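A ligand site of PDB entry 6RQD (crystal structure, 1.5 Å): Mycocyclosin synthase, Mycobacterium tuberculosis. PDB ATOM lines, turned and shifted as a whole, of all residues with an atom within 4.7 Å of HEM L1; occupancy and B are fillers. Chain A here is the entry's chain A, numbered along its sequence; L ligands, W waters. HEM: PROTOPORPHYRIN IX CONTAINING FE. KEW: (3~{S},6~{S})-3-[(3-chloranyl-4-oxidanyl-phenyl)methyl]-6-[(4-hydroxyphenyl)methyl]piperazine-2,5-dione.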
ATOM      1  N   MET A  62      -8.301 -23.154 -30.919  1.00  0.00           N
ATOM      2  CA  MET A  62      -7.184 -23.709 -30.146  1.00  0.00           C
ATOM      3  C   MET A  62      -6.296 -24.552 -31.046  1.00  0.00           C
ATOM      4  O   MET A  62      -5.063 -24.399 -31.049  1.00  0.00           O
ATOM      5  CB  MET A  62      -7.687 -24.539 -28.953  1.00  0.00           C
ATOM      6  CG  MET A  62      -6.607 -25.462 -28.327  1.00  0.00           C
ATOM      7  SD  MET A  62      -7.149 -26.476 -26.930  1.00  0.00           S
ATOM      8  CE  MET A  62      -7.573 -25.158 -25.808  1.00  0.00           C
ATOM      9  N   MET A  86      -8.742 -32.922 -27.090  1.00  0.00           N
ATOM     10  CA  MET A  86     -10.159 -33.189 -26.912  1.00  0.00           C
ATOM     11  C   MET A  86     -10.831 -33.520 -28.236  1.00  0.00           C
ATOM     12  O   MET A  86     -11.737 -34.367 -28.289  1.00  0.00           O
ATOM     13  CB  MET A  86     -10.868 -32.023 -26.219  1.00  0.00           C
ATOM     14  CG  MET A  86     -10.583 -31.882 -24.733  1.00  0.00           C
ATOM     15  SD  MET A  86     -10.907 -33.318 -23.675  1.00  0.00           S
ATOM     16  CE  MET A  86     -12.609 -33.716 -24.056  1.00  0.00           C
ATOM     17  N   ILE A 102     -13.927 -39.244 -14.905  1.00  0.00           N
ATOM     18  CA  ILE A 102     -13.294 -38.194 -14.118  1.00  0.00           C
ATOM     19  C   ILE A 102     -14.313 -37.423 -13.287  1.00  0.00           C
ATOM     20  O   ILE A 102     -14.039 -36.317 -12.830  1.00  0.00           O
ATOM     21  CB  ILE A 102     -12.420 -37.261 -14.973  1.00  0.00           C
ATOM     22  CG1 ILE A 102     -13.269 -36.508 -15.990  1.00  0.00           C
ATOM     23  CG2 ILE A 102     -11.327 -38.054 -15.674  1.00  0.00           C
ATOM     24  CD1 ILE A 102     -12.505 -35.451 -16.771  1.00  0.00           C
ATOM     25  N   HIS A 146      -5.436 -37.951  -8.607  1.00  0.00           N
ATOM     26  CA  HIS A 146      -5.362 -38.326 -10.017  1.00  0.00           C
ATOM     27  C   HIS A 146      -4.894 -39.767 -10.218  1.00  0.00           C
ATOM     28  O   HIS A 146      -5.326 -40.416 -11.172  1.00  0.00           O
ATOM     29  CB  HIS A 146      -4.606 -37.293 -10.819  1.00  0.00           C
ATOM     30  CG  HIS A 146      -5.409 -36.055 -11.029  1.00  0.00           C
ATOM     31  ND1 HIS A 146      -5.527 -35.081 -10.061  1.00  0.00           N
ATOM     32  CD2 HIS A 146      -6.217 -35.672 -12.051  1.00  0.00           C
ATOM     33  CE1 HIS A 146      -6.334 -34.126 -10.491  1.00  0.00           C
ATOM     34  NE2 HIS A 146      -6.768 -34.461 -11.696  1.00  0.00           N
ATOM     35  N   PHE A 230      -4.322 -36.208 -19.041  1.00  0.00           N
ATOM     36  CA  PHE A 230      -5.295 -35.966 -17.985  1.00  0.00           C
ATOM     37  C   PHE A 230      -4.646 -35.982 -16.611  1.00  0.00           C
ATOM     38  O   PHE A 230      -5.044 -35.219 -15.730  1.00  0.00           O
ATOM     39  CB  PHE A 230      -6.485 -36.912 -18.073  1.00  0.00           C
ATOM     40  CG  PHE A 230      -7.561 -36.400 -18.987  1.00  0.00           C
ATOM     41  CD1 PHE A 230      -7.338 -36.355 -20.355  1.00  0.00           C
ATOM     42  CD2 PHE A 230      -8.758 -35.914 -18.491  1.00  0.00           C
ATOM     43  CE1 PHE A 230      -8.301 -35.864 -21.223  1.00  0.00           C
ATOM     44  CE2 PHE A 230      -9.743 -35.425 -19.356  1.00  0.00           C
ATOM     45  CZ  PHE A 230      -9.497 -35.403 -20.728  1.00  0.00           C
ATOM     46  N   ALA A 233      -2.519 -32.260 -16.814  1.00  0.00           N
ATOM     47  CA  ALA A 233      -3.396 -31.104 -16.704  1.00  0.00           C
ATOM     48  C   ALA A 233      -4.170 -31.121 -15.394  1.00  0.00           C
ATOM     49  O   ALA A 233      -4.306 -30.082 -14.725  1.00  0.00           O
ATOM     50  CB  ALA A 233      -4.348 -31.073 -17.907  1.00  0.00           C
ATOM     51  N   GLY A 234      -4.686 -32.285 -14.991  1.00  0.00           N
ATOM     52  CA  GLY A 234      -5.448 -32.356 -13.759  1.00  0.00           C
ATOM     53  C   GLY A 234      -4.608 -32.008 -12.534  1.00  0.00           C
ATOM     54  O   GLY A 234      -5.011 -31.204 -11.703  1.00  0.00           O
ATOM     55  N   SER A 237      -3.314 -28.376 -12.505  1.00  0.00           N
ATOM     56  CA  SER A 237      -4.401 -27.413 -12.369  1.00  0.00           C
ATOM     57  C   SER A 237      -4.981 -27.430 -10.958  1.00  0.00           C
ATOM     58  O   SER A 237      -5.174 -26.374 -10.353  1.00  0.00           O
ATOM     59  CB  SER A 237      -5.479 -27.664 -13.423  1.00  0.00           C
ATOM     60  OG  SER A 237      -4.947 -27.403 -14.710  1.00  0.00           O
ATOM     61  N   THR A 238      -5.271 -28.623 -10.412  1.00  0.00           N
ATOM     62  CA  THR A 238      -5.856 -28.680  -9.071  1.00  0.00           C
ATOM     63  C   THR A 238      -4.841 -28.313  -7.991  1.00  0.00           C
ATOM     64  O   THR A 238      -5.167 -27.596  -7.048  1.00  0.00           O
ATOM     65  CB  THR A 238      -6.455 -30.059  -8.783  1.00  0.00           C
ATOM     66  OG1 THR A 238      -5.447 -31.074  -8.918  1.00  0.00           O
ATOM     67  CG2 THR A 238      -7.637 -30.363  -9.711  1.00  0.00           C
ATOM     68  N   PHE A 241      -4.328 -24.452  -8.278  1.00  0.00           N
ATOM     69  CA  PHE A 241      -5.489 -23.715  -7.805  1.00  0.00           C
ATOM     70  C   PHE A 241      -5.623 -23.811  -6.276  1.00  0.00           C
ATOM     71  O   PHE A 241      -5.847 -22.800  -5.593  1.00  0.00           O
ATOM     72  CB  PHE A 241      -6.803 -24.176  -8.450  1.00  0.00           C
ATOM     73  CG  PHE A 241      -7.997 -23.603  -7.761  1.00  0.00           C
ATOM     74  CD1 PHE A 241      -8.226 -22.240  -7.794  1.00  0.00           C
ATOM     75  CD2 PHE A 241      -8.838 -24.393  -6.993  1.00  0.00           C
ATOM     76  CE1 PHE A 241      -9.279 -21.686  -7.108  1.00  0.00           C
ATOM     77  CE2 PHE A 241      -9.891 -23.839  -6.307  1.00  0.00           C
ATOM     78  CZ  PHE A 241     -10.116 -22.484  -6.371  1.00  0.00           C
ATOM     79  N   LEU A 274     -12.263 -19.587  -6.960  1.00  0.00           N
ATOM     80  CA  LEU A 274     -12.051 -19.827  -8.381  1.00  0.00           C
ATOM     81  C   LEU A 274     -12.111 -18.532  -9.168  1.00  0.00           C
ATOM     82  O   LEU A 274     -11.254 -18.249 -10.010  1.00  0.00           O
ATOM     83  CB  LEU A 274     -13.100 -20.806  -8.904  1.00  0.00           C
ATOM     84  CG  LEU A 274     -12.865 -22.272  -8.588  1.00  0.00           C
ATOM     85  CD1 LEU A 274     -14.159 -23.066  -8.800  1.00  0.00           C
ATOM     86  CD2 LEU A 274     -11.719 -22.838  -9.425  1.00  0.00           C
ATOM     87  N   PHE A 280      -3.675 -19.259 -13.692  1.00  0.00           N
ATOM     88  CA  PHE A 280      -3.226 -19.295 -15.082  1.00  0.00           C
ATOM     89  C   PHE A 280      -2.316 -18.103 -15.351  1.00  0.00           C
ATOM     90  O   PHE A 280      -2.745 -16.940 -15.247  1.00  0.00           O
ATOM     91  CB  PHE A 280      -4.376 -19.330 -16.084  1.00  0.00           C
ATOM     92  CG  PHE A 280      -4.872 -20.719 -16.388  1.00  0.00           C
ATOM     93  CD1 PHE A 280      -5.482 -21.476 -15.407  1.00  0.00           C
ATOM     94  CD2 PHE A 280      -4.722 -21.272 -17.658  1.00  0.00           C
ATOM     95  CE1 PHE A 280      -5.929 -22.770 -15.671  1.00  0.00           C
ATOM     96  CE2 PHE A 280      -5.190 -22.559 -17.933  1.00  0.00           C
ATOM     97  CZ  PHE A 280      -5.797 -23.308 -16.934  1.00  0.00           C
ATOM     98  N   LEU A 284      -5.394 -17.372 -22.336  1.00  0.00           N
ATOM     99  CA  LEU A 284      -5.630 -18.584 -23.127  1.00  0.00           C
ATOM    100  C   LEU A 284      -5.435 -18.267 -24.594  1.00  0.00           C
ATOM    101  O   LEU A 284      -6.019 -17.313 -25.101  1.00  0.00           O
ATOM    102  CB  LEU A 284      -7.060 -19.101 -22.930  1.00  0.00           C
ATOM    103  CG  LEU A 284      -7.465 -19.404 -21.492  1.00  0.00           C
ATOM    104  CD1 LEU A 284      -8.900 -19.913 -21.451  1.00  0.00           C
ATOM    105  CD2 LEU A 284      -6.548 -20.420 -20.856  1.00  0.00           C
ATOM    106  N   ARG A 286      -5.639 -18.487 -28.753  1.00  0.00           N
ATOM    107  CA  ARG A 286      -6.458 -18.878 -29.887  1.00  0.00           C
ATOM    108  C   ARG A 286      -5.871 -18.248 -31.140  1.00  0.00           C
ATOM    109  O   ARG A 286      -5.297 -17.159 -31.084  1.00  0.00           O
ATOM    110  CB  ARG A 286      -7.892 -18.382 -29.688  1.00  0.00           C
ATOM    111  CG  ARG A 286      -8.608 -18.971 -28.465  1.00  0.00           C
ATOM    112  CD  ARG A 286      -8.838 -20.462 -28.592  1.00  0.00           C
ATOM    113  NE  ARG A 286      -9.787 -20.982 -27.603  1.00  0.00           N
ATOM    114  CZ  ARG A 286      -9.446 -21.496 -26.421  1.00  0.00           C
ATOM    115  NH1 ARG A 286      -8.173 -21.553 -26.078  1.00  0.00           N
ATOM    116  NH2 ARG A 286     -10.381 -21.960 -25.600  1.00  0.00           N
ATOM    117  N   LEU A 309      -7.863 -14.406 -18.347  1.00  0.00           N
ATOM    118  CA  LEU A 309      -8.944 -14.848 -17.469  1.00  0.00           C
ATOM    119  C   LEU A 309      -9.198 -13.861 -16.333  1.00  0.00           C
ATOM    120  O   LEU A 309     -10.359 -13.601 -16.000  1.00  0.00           O
ATOM    121  CB  LEU A 309      -8.635 -16.241 -16.921  1.00  0.00           C
ATOM    122  CG  LEU A 309      -8.562 -17.377 -17.956  1.00  0.00           C
ATOM    123  CD1 LEU A 309      -8.332 -18.729 -17.271  1.00  0.00           C
ATOM    124  CD2 LEU A 309      -9.793 -17.427 -18.841  1.00  0.00           C
ATOM    125  N   LEU A 336     -14.801 -17.288 -15.574  1.00  0.00           N
ATOM    126  CA  LEU A 336     -14.106 -18.030 -16.619  1.00  0.00           C
ATOM    127  C   LEU A 336     -12.931 -18.858 -16.080  1.00  0.00           C
ATOM    128  O   LEU A 336     -12.027 -19.214 -16.848  1.00  0.00           O
ATOM    129  CB  LEU A 336     -13.620 -17.085 -17.725  1.00  0.00           C
ATOM    130  CG  LEU A 336     -14.647 -16.109 -18.295  1.00  0.00           C
ATOM    131  CD1 LEU A 336     -14.105 -15.375 -19.519  1.00  0.00           C
ATOM    132  CD2 LEU A 336     -15.954 -16.792 -18.639  1.00  0.00           C
ATOM    133  N   ALA A 337     -12.950 -19.228 -14.793  1.00  0.00           N
ATOM    134  CA  ALA A 337     -11.835 -19.976 -14.235  1.00  0.00           C
ATOM    135  C   ALA A 337     -11.625 -21.315 -14.943  1.00  0.00           C
ATOM    136  O   ALA A 337     -10.490 -21.801 -15.002  1.00  0.00           O
ATOM    137  CB  ALA A 337     -12.036 -20.213 -12.735  1.00  0.00           C
ATOM    138  N   PHE A 338     -12.699 -21.920 -15.444  1.00  0.00           N
ATOM    139  CA  PHE A 338     -12.629 -23.167 -16.201  1.00  0.00           C
ATOM    140  C   PHE A 338     -12.745 -22.942 -17.702  1.00  0.00           C
ATOM    141  O   PHE A 338     -12.972 -23.901 -18.459  1.00  0.00           O
ATOM    142  CB  PHE A 338     -13.741 -24.128 -15.758  1.00  0.00           C
ATOM    143  CG  PHE A 338     -13.592 -24.632 -14.343  1.00  0.00           C
ATOM    144  CD1 PHE A 338     -12.507 -25.411 -13.975  1.00  0.00           C
ATOM    145  CD2 PHE A 338     -14.545 -24.329 -13.370  1.00  0.00           C
ATOM    146  CE1 PHE A 338     -12.368 -25.875 -12.684  1.00  0.00           C
ATOM    147  CE2 PHE A 338     -14.414 -24.797 -12.076  1.00  0.00           C
ATOM    148  CZ  PHE A 338     -13.324 -25.580 -11.729  1.00  0.00           C
ATOM    149  N   GLY A 339     -12.596 -21.715 -18.163  1.00  0.00           N
ATOM    150  CA  GLY A 339     -12.775 -21.438 -19.567  1.00  0.00           C
ATOM    151  C   GLY A 339     -14.242 -21.305 -19.933  1.00  0.00           C
ATOM    152  O   GLY A 339     -15.103 -21.077 -19.075  1.00  0.00           O
ATOM    153  N   GLN A 342     -16.142 -24.291 -26.482  1.00  0.00           N
ATOM    154  CA  GLN A 342     -15.772 -25.615 -26.969  1.00  0.00           C
ATOM    155  C   GLN A 342     -14.802 -26.312 -26.027  1.00  0.00           C
ATOM    156  O   GLN A 342     -14.879 -27.527 -25.833  1.00  0.00           O
ATOM    157  CB  GLN A 342     -15.153 -25.478 -28.360  1.00  0.00           C
ATOM    158  CG  GLN A 342     -14.719 -26.783 -28.997  1.00  0.00           C
ATOM    159  CD  GLN A 342     -15.887 -27.647 -29.418  1.00  0.00           C
ATOM    160  OE1 GLN A 342     -17.028 -27.185 -29.501  1.00  0.00           O
ATOM    161  NE2 GLN A 342     -15.613 -28.924 -29.680  1.00  0.00           N
ATOM    162  N   HIS A 343     -13.883 -25.565 -25.419  1.00  0.00           N
ATOM    163  CA  HIS A 343     -12.791 -26.133 -24.637  1.00  0.00           C
ATOM    164  C   HIS A 343     -12.973 -25.961 -23.137  1.00  0.00           C
ATOM    165  O   HIS A 343     -11.988 -26.042 -22.390  1.00  0.00           O
ATOM    166  CB  HIS A 343     -11.460 -25.580 -25.140  1.00  0.00           C
ATOM    167  CG  HIS A 343     -11.167 -25.952 -26.563  1.00  0.00           C
ATOM    168  ND1 HIS A 343     -10.705 -27.199 -26.921  1.00  0.00           N
ATOM    169  CD2 HIS A 343     -11.296 -25.252 -27.713  1.00  0.00           C
ATOM    170  CE1 HIS A 343     -10.550 -27.253 -28.227  1.00  0.00           C
ATOM    171  NE2 HIS A 343     -10.902 -26.087 -28.738  1.00  0.00           N
ATOM    172  N   CYS A 345     -13.302 -26.698 -19.370  1.00  0.00           N
ATOM    173  CA  CYS A 345     -12.590 -27.732 -18.640  1.00  0.00           C
ATOM    174  C   CYS A 345     -13.469 -28.962 -18.437  1.00  0.00           C
ATOM    175  O   CYS A 345     -14.563 -28.852 -17.855  1.00  0.00           O
ATOM    176  CB  CYS A 345     -12.164 -27.203 -17.274  1.00  0.00           C
ATOM    177  SG  CYS A 345     -11.286 -28.442 -16.330  1.00  0.00           S
ATOM    178  N   PRO A 346     -13.039 -30.147 -18.883  1.00  0.00           N
ATOM    179  CA  PRO A 346     -13.831 -31.359 -18.646  1.00  0.00           C
ATOM    180  C   PRO A 346     -13.733 -31.894 -17.221  1.00  0.00           C
ATOM    181  O   PRO A 346     -14.522 -32.783 -16.868  1.00  0.00           O
ATOM    182  CB  PRO A 346     -13.245 -32.360 -19.653  1.00  0.00           C
ATOM    183  CG  PRO A 346     -11.797 -31.959 -19.748  1.00  0.00           C
ATOM    184  CD  PRO A 346     -11.802 -30.434 -19.654  1.00  0.00           C
ATOM    185  N   GLY A 347     -12.810 -31.386 -16.404  1.00  0.00           N
ATOM    186  CA  GLY A 347     -12.649 -31.863 -15.045  1.00  0.00           C
ATOM    187  C   GLY A 347     -13.126 -30.876 -13.995  1.00  0.00           C
ATOM    188  O   GLY A 347     -12.720 -30.970 -12.835  1.00  0.00           O
ATOM    189  N   LEU A 350     -14.498 -32.191 -10.668  1.00  0.00           N
ATOM    190  CA  LEU A 350     -13.472 -32.825  -9.837  1.00  0.00           C
ATOM    191  C   LEU A 350     -12.525 -31.802  -9.240  1.00  0.00           C
ATOM    192  O   LEU A 350     -12.079 -31.964  -8.102  1.00  0.00           O
ATOM    193  CB  LEU A 350     -12.693 -33.812 -10.693  1.00  0.00           C
ATOM    194  CG  LEU A 350     -11.682 -34.704  -9.982  1.00  0.00           C
ATOM    195  CD1 LEU A 350     -12.360 -35.634  -9.016  1.00  0.00           C
ATOM    196  CD2 LEU A 350     -10.914 -35.476 -11.036  1.00  0.00           C
ATOM    197  N   GLY A 351     -12.188 -30.756  -9.994  1.00  0.00           N
ATOM    198  CA  GLY A 351     -11.391 -29.685  -9.439  1.00  0.00           C
ATOM    199  C   GLY A 351     -12.092 -28.978  -8.302  1.00  0.00           C
ATOM    200  O   GLY A 351     -11.480 -28.627  -7.295  1.00  0.00           O
HETATM  201  CHA HEM L   1      -9.019 -27.196 -19.854  1.00  0.00           C
HETATM  202  CHB HEM L   1      -8.833 -24.809 -15.736  1.00  0.00           C
HETATM  203  CHC HEM L   1      -8.989 -29.055 -13.349  1.00  0.00           C
HETATM  204  CHD HEM L   1      -8.241 -31.335 -17.503  1.00  0.00           C
HETATM  205  C1A HEM L   1      -9.052 -26.194 -18.933  1.00  0.00           C
HETATM  206  C2A HEM L   1      -9.188 -24.818 -19.271  1.00  0.00           C
HETATM  207  C3A HEM L   1      -9.122 -24.152 -18.093  1.00  0.00           C
HETATM  208  C4A HEM L   1      -8.939 -25.104 -17.064  1.00  0.00           C
HETATM  209  CMA HEM L   1      -9.221 -22.665 -17.924  1.00  0.00           C
HETATM  210  CAA HEM L   1      -9.433 -24.242 -20.647  1.00  0.00           C
HETATM  211  CBA HEM L   1      -8.162 -24.003 -21.470  1.00  0.00           C
HETATM  212  CGA HEM L   1      -8.432 -23.310 -22.781  1.00  0.00           C
HETATM  213  O1A HEM L   1      -9.610 -23.092 -23.086  1.00  0.00           O
HETATM  214  O2A HEM L   1      -7.489 -22.953 -23.449  1.00  0.00           O
HETATM  215  C1B HEM L   1      -8.844 -25.776 -14.704  1.00  0.00           C
HETATM  216  C2B HEM L   1      -8.805 -25.464 -13.341  1.00  0.00           C
HETATM  217  C3B HEM L   1      -8.852 -26.645 -12.673  1.00  0.00           C
HETATM  218  C4B HEM L   1      -8.903 -27.701 -13.668  1.00  0.00           C
HETATM  219  CMB HEM L   1      -8.755 -24.097 -12.728  1.00  0.00           C
HETATM  220  CAB HEM L   1      -8.843 -26.929 -11.252  1.00  0.00           C
HETATM  221  CBB HEM L   1      -9.472 -26.216 -10.359  1.00  0.00           C
HETATM  222  C1C HEM L   1      -8.839 -30.086 -14.254  1.00  0.00           C
HETATM  223  C2C HEM L   1      -8.866 -31.457 -13.992  1.00  0.00           C
HETATM  224  C3C HEM L   1      -8.653 -32.054 -15.220  1.00  0.00           C
HETATM  225  C4C HEM L   1      -8.490 -31.052 -16.181  1.00  0.00           C
HETATM  226  CMC HEM L   1      -9.101 -32.074 -12.645  1.00  0.00           C
HETATM  227  CAC HEM L   1      -8.577 -33.468 -15.537  1.00  0.00           C
HETATM  228  CBC HEM L   1      -8.733 -34.378 -14.616  1.00  0.00           C
HETATM  229  C1D HEM L   1      -8.354 -30.351 -18.457  1.00  0.00           C
HETATM  230  C2D HEM L   1      -8.189 -30.657 -19.877  1.00  0.00           C
HETATM  231  C3D HEM L   1      -8.395 -29.499 -20.517  1.00  0.00           C
HETATM  232  C4D HEM L   1      -8.707 -28.489 -19.502  1.00  0.00           C
HETATM  233  CMD HEM L   1      -7.803 -31.986 -20.452  1.00  0.00           C
HETATM  234  CAD HEM L   1      -8.301 -29.254 -22.004  1.00  0.00           C
HETATM  235  CBD HEM L   1      -9.664 -29.268 -22.620  1.00  0.00           C
HETATM  236  CGD HEM L   1      -9.534 -29.089 -24.074  1.00  0.00           C
HETATM  237  O1D HEM L   1     -10.549 -28.914 -24.736  1.00  0.00           O
HETATM  238  O2D HEM L   1      -8.473 -29.049 -24.660  1.00  0.00           O
HETATM  239  NA  HEM L   1      -8.905 -26.331 -17.606  1.00  0.00           N
HETATM  240  NB  HEM L   1      -8.902 -27.062 -14.813  1.00  0.00           N
HETATM  241  NC  HEM L   1      -8.646 -29.889 -15.550  1.00  0.00           N
HETATM  242  ND  HEM L   1      -8.764 -29.122 -18.340  1.00  0.00           N
HETATM  243 FE   HEM L   1      -8.988 -28.116 -16.625  1.00  0.00          FE
HETATM  244  C02 KEW L   2      -3.213 -26.563 -20.589  1.00  0.00           C
HETATM  245  C03 KEW L   2      -2.527 -26.349 -21.759  1.00  0.00           C
HETATM  246  C04 KEW L   2      -3.090 -26.600 -22.903  1.00  0.00           C
HETATM  247  C05 KEW L   2      -4.367 -27.138 -22.930  1.00  0.00           C
HETATM  248  C06 KEW L   2      -5.008 -27.430 -24.275  1.00  0.00           C
HETATM  249  C07 KEW L   2      -4.588 -28.754 -24.945  1.00  0.00           C
HETATM  250  C08 KEW L   2      -3.047 -29.039 -24.975  1.00  0.00           C
HETATM  251  C10 KEW L   2      -3.220 -30.762 -23.262  1.00  0.00           C
HETATM  252  C11 KEW L   2      -2.862 -30.427 -21.781  1.00  0.00           C
HETATM  253  C12 KEW L   2      -1.474 -30.823 -21.457  1.00  0.00           C
HETATM  254  C13 KEW L   2      -0.411 -30.063 -21.808  1.00  0.00           C
HETATM  255  C14 KEW L   2       0.906 -30.444 -21.523  1.00  0.00           C
HETATM  256  C15 KEW L   2       1.113 -31.651 -20.917  1.00  0.00           C
HETATM  257  C17 KEW L   2       0.045 -32.407 -20.544  1.00  0.00           C
HETATM  258  C18 KEW L   2      -1.213 -31.996 -20.818  1.00  0.00           C
HETATM  259  C19 KEW L   2      -4.704 -30.762 -23.547  1.00  0.00           C
HETATM  260  C23 KEW L   2      -5.026 -27.306 -21.750  1.00  0.00           C
HETATM  261  C24 KEW L   2      -4.404 -26.977 -20.560  1.00  0.00           C
HETATM  262  N09 KEW L   2      -2.509 -29.991 -24.177  1.00  0.00           N
HETATM  263  N20 KEW L   2      -5.295 -29.855 -24.297  1.00  0.00           N
HETATM  264  O01 KEW L   2      -2.651 -26.282 -19.468  1.00  0.00           O
HETATM  265  O16 KEW L   2       2.355 -32.042 -20.626  1.00  0.00           O
HETATM  266  O21 KEW L   2      -5.388 -31.636 -23.053  1.00  0.00           O
HETATM  267  O22 KEW L   2      -2.290 -28.414 -25.661  1.00  0.00           O
HETATM  268 CL1  KEW L   2      -5.052 -27.169 -19.010  1.00  0.00          CL
HETATM  269  O   HOH W   1     -12.233 -22.765 -22.599  1.00  0.00           O
HETATM  270  O   HOH W   2     -13.053 -29.753 -23.252  1.00  0.00           O
HETATM  271  O   HOH W   3      -5.012 -23.570 -22.992  1.00  0.00           O
HETATM  272  O   HOH W   4      -6.540 -27.908 -16.783  1.00  0.00           O
HETATM  273  O   HOH W   5      -7.782 -30.063 -27.014  1.00  0.00           O
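O1A of HEM L1 is in salt-bridge range of NH2 of Arg 286. O1D of HEM L1 is in hydrogen-bond range of ND1 of His 343. An iron atom (FE) of HEM L1 is bound by the side-chain sulfur (SG) of Cys 345, 2.3 Å away.
A nitrogen (N20) of KEW L2 is in hydrogen-bond range of an oxygen (O2D) of HEM L1, 3.3 Å away.
The side-chain hydroxyl (OG1) of Thr 238 lies within hydrogen-bond range of the backbone carbonyl oxygen (O) of Gly 234, at 2.8 Å. The side-chain hydroxyl of Ser 237 lies within hydrogen-bond range of the backbone carbonyl oxygen of Ala 233. N of Gly 347 lies close to SG of Cys 345 (3.3 Å). A ring nitrogen (ND1) of His 343 is in hydrogen-bond range of the side-chain sulfur of Met 62 (3.6 Å). The backbone NH (N) of Cys 345 lies within hydrogen-bond range of the backbone carbonyl oxygen (O) of Phe 338 (3.0 Å).
SD of Met 62 lies close to O2D of HEM L1 (3.7 Å). Met 86 touches HEM L1. His 146 touches HEM L1 (NE2 to CMC, 3.5 Å). Phe 230 touches HEM L1. Ala 233 touches HEM L1 (CB to CHD, 3.9 Å). CA of Gly 234 touches C3C of HEM L1, 3.5 Å away. Ser 237 touches HEM L1 (CB to C4B, 3.4 Å). Thr 238 touches HEM L1 (CG2 to CMC, 3.7 Å). Phe 241 touches HEM L1. Phe 280 touches HEM L1 (CE1 to CHB, 3.5 Å). Leu 284 touches HEM L1 (CD1 to O1A, 3.6 Å). O of Ala 337 touches CMA of HEM L1, at 3.3 Å. Phe 338 touches HEM L1 (C to CMA, 3.5 Å). N of Gly 339 touches CMA of HEM L1 (3.5 Å). Pro 346 touches HEM L1 (CD to ND, 3.6 Å). Gly 347 touches HEM L1. Hydrophobic or aromatic side chains that line HEM L1: Met 62, Met 86, His 146, Phe 230, Ala 233, Phe 241, Phe 280, Leu 284, Phe 338, His 343 and Pro 346. Within 4 Å of HEM L1: Met 62, Met 86, His 146, Phe 230, Ala 233, Gly 234, Ser 237, Thr 238, Phe 241, Phe 280, Leu 284, Arg 286, Ala 337, Phe 338, Gly 339, His 343, Cys 345, Pro 346 and Gly 347. The nearest printed residue that does not touch HEM L1 is Gly 351 (4.1 Å).
Water W5 lies within hydrogen-bond range of O2D of HEM L1, N of Met 86 and SD of Met 62. Water W1 lies within hydrogen-bond range of an oxygen (O1A) of HEM L1 and the backbone carbonyl oxygen of His 343.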
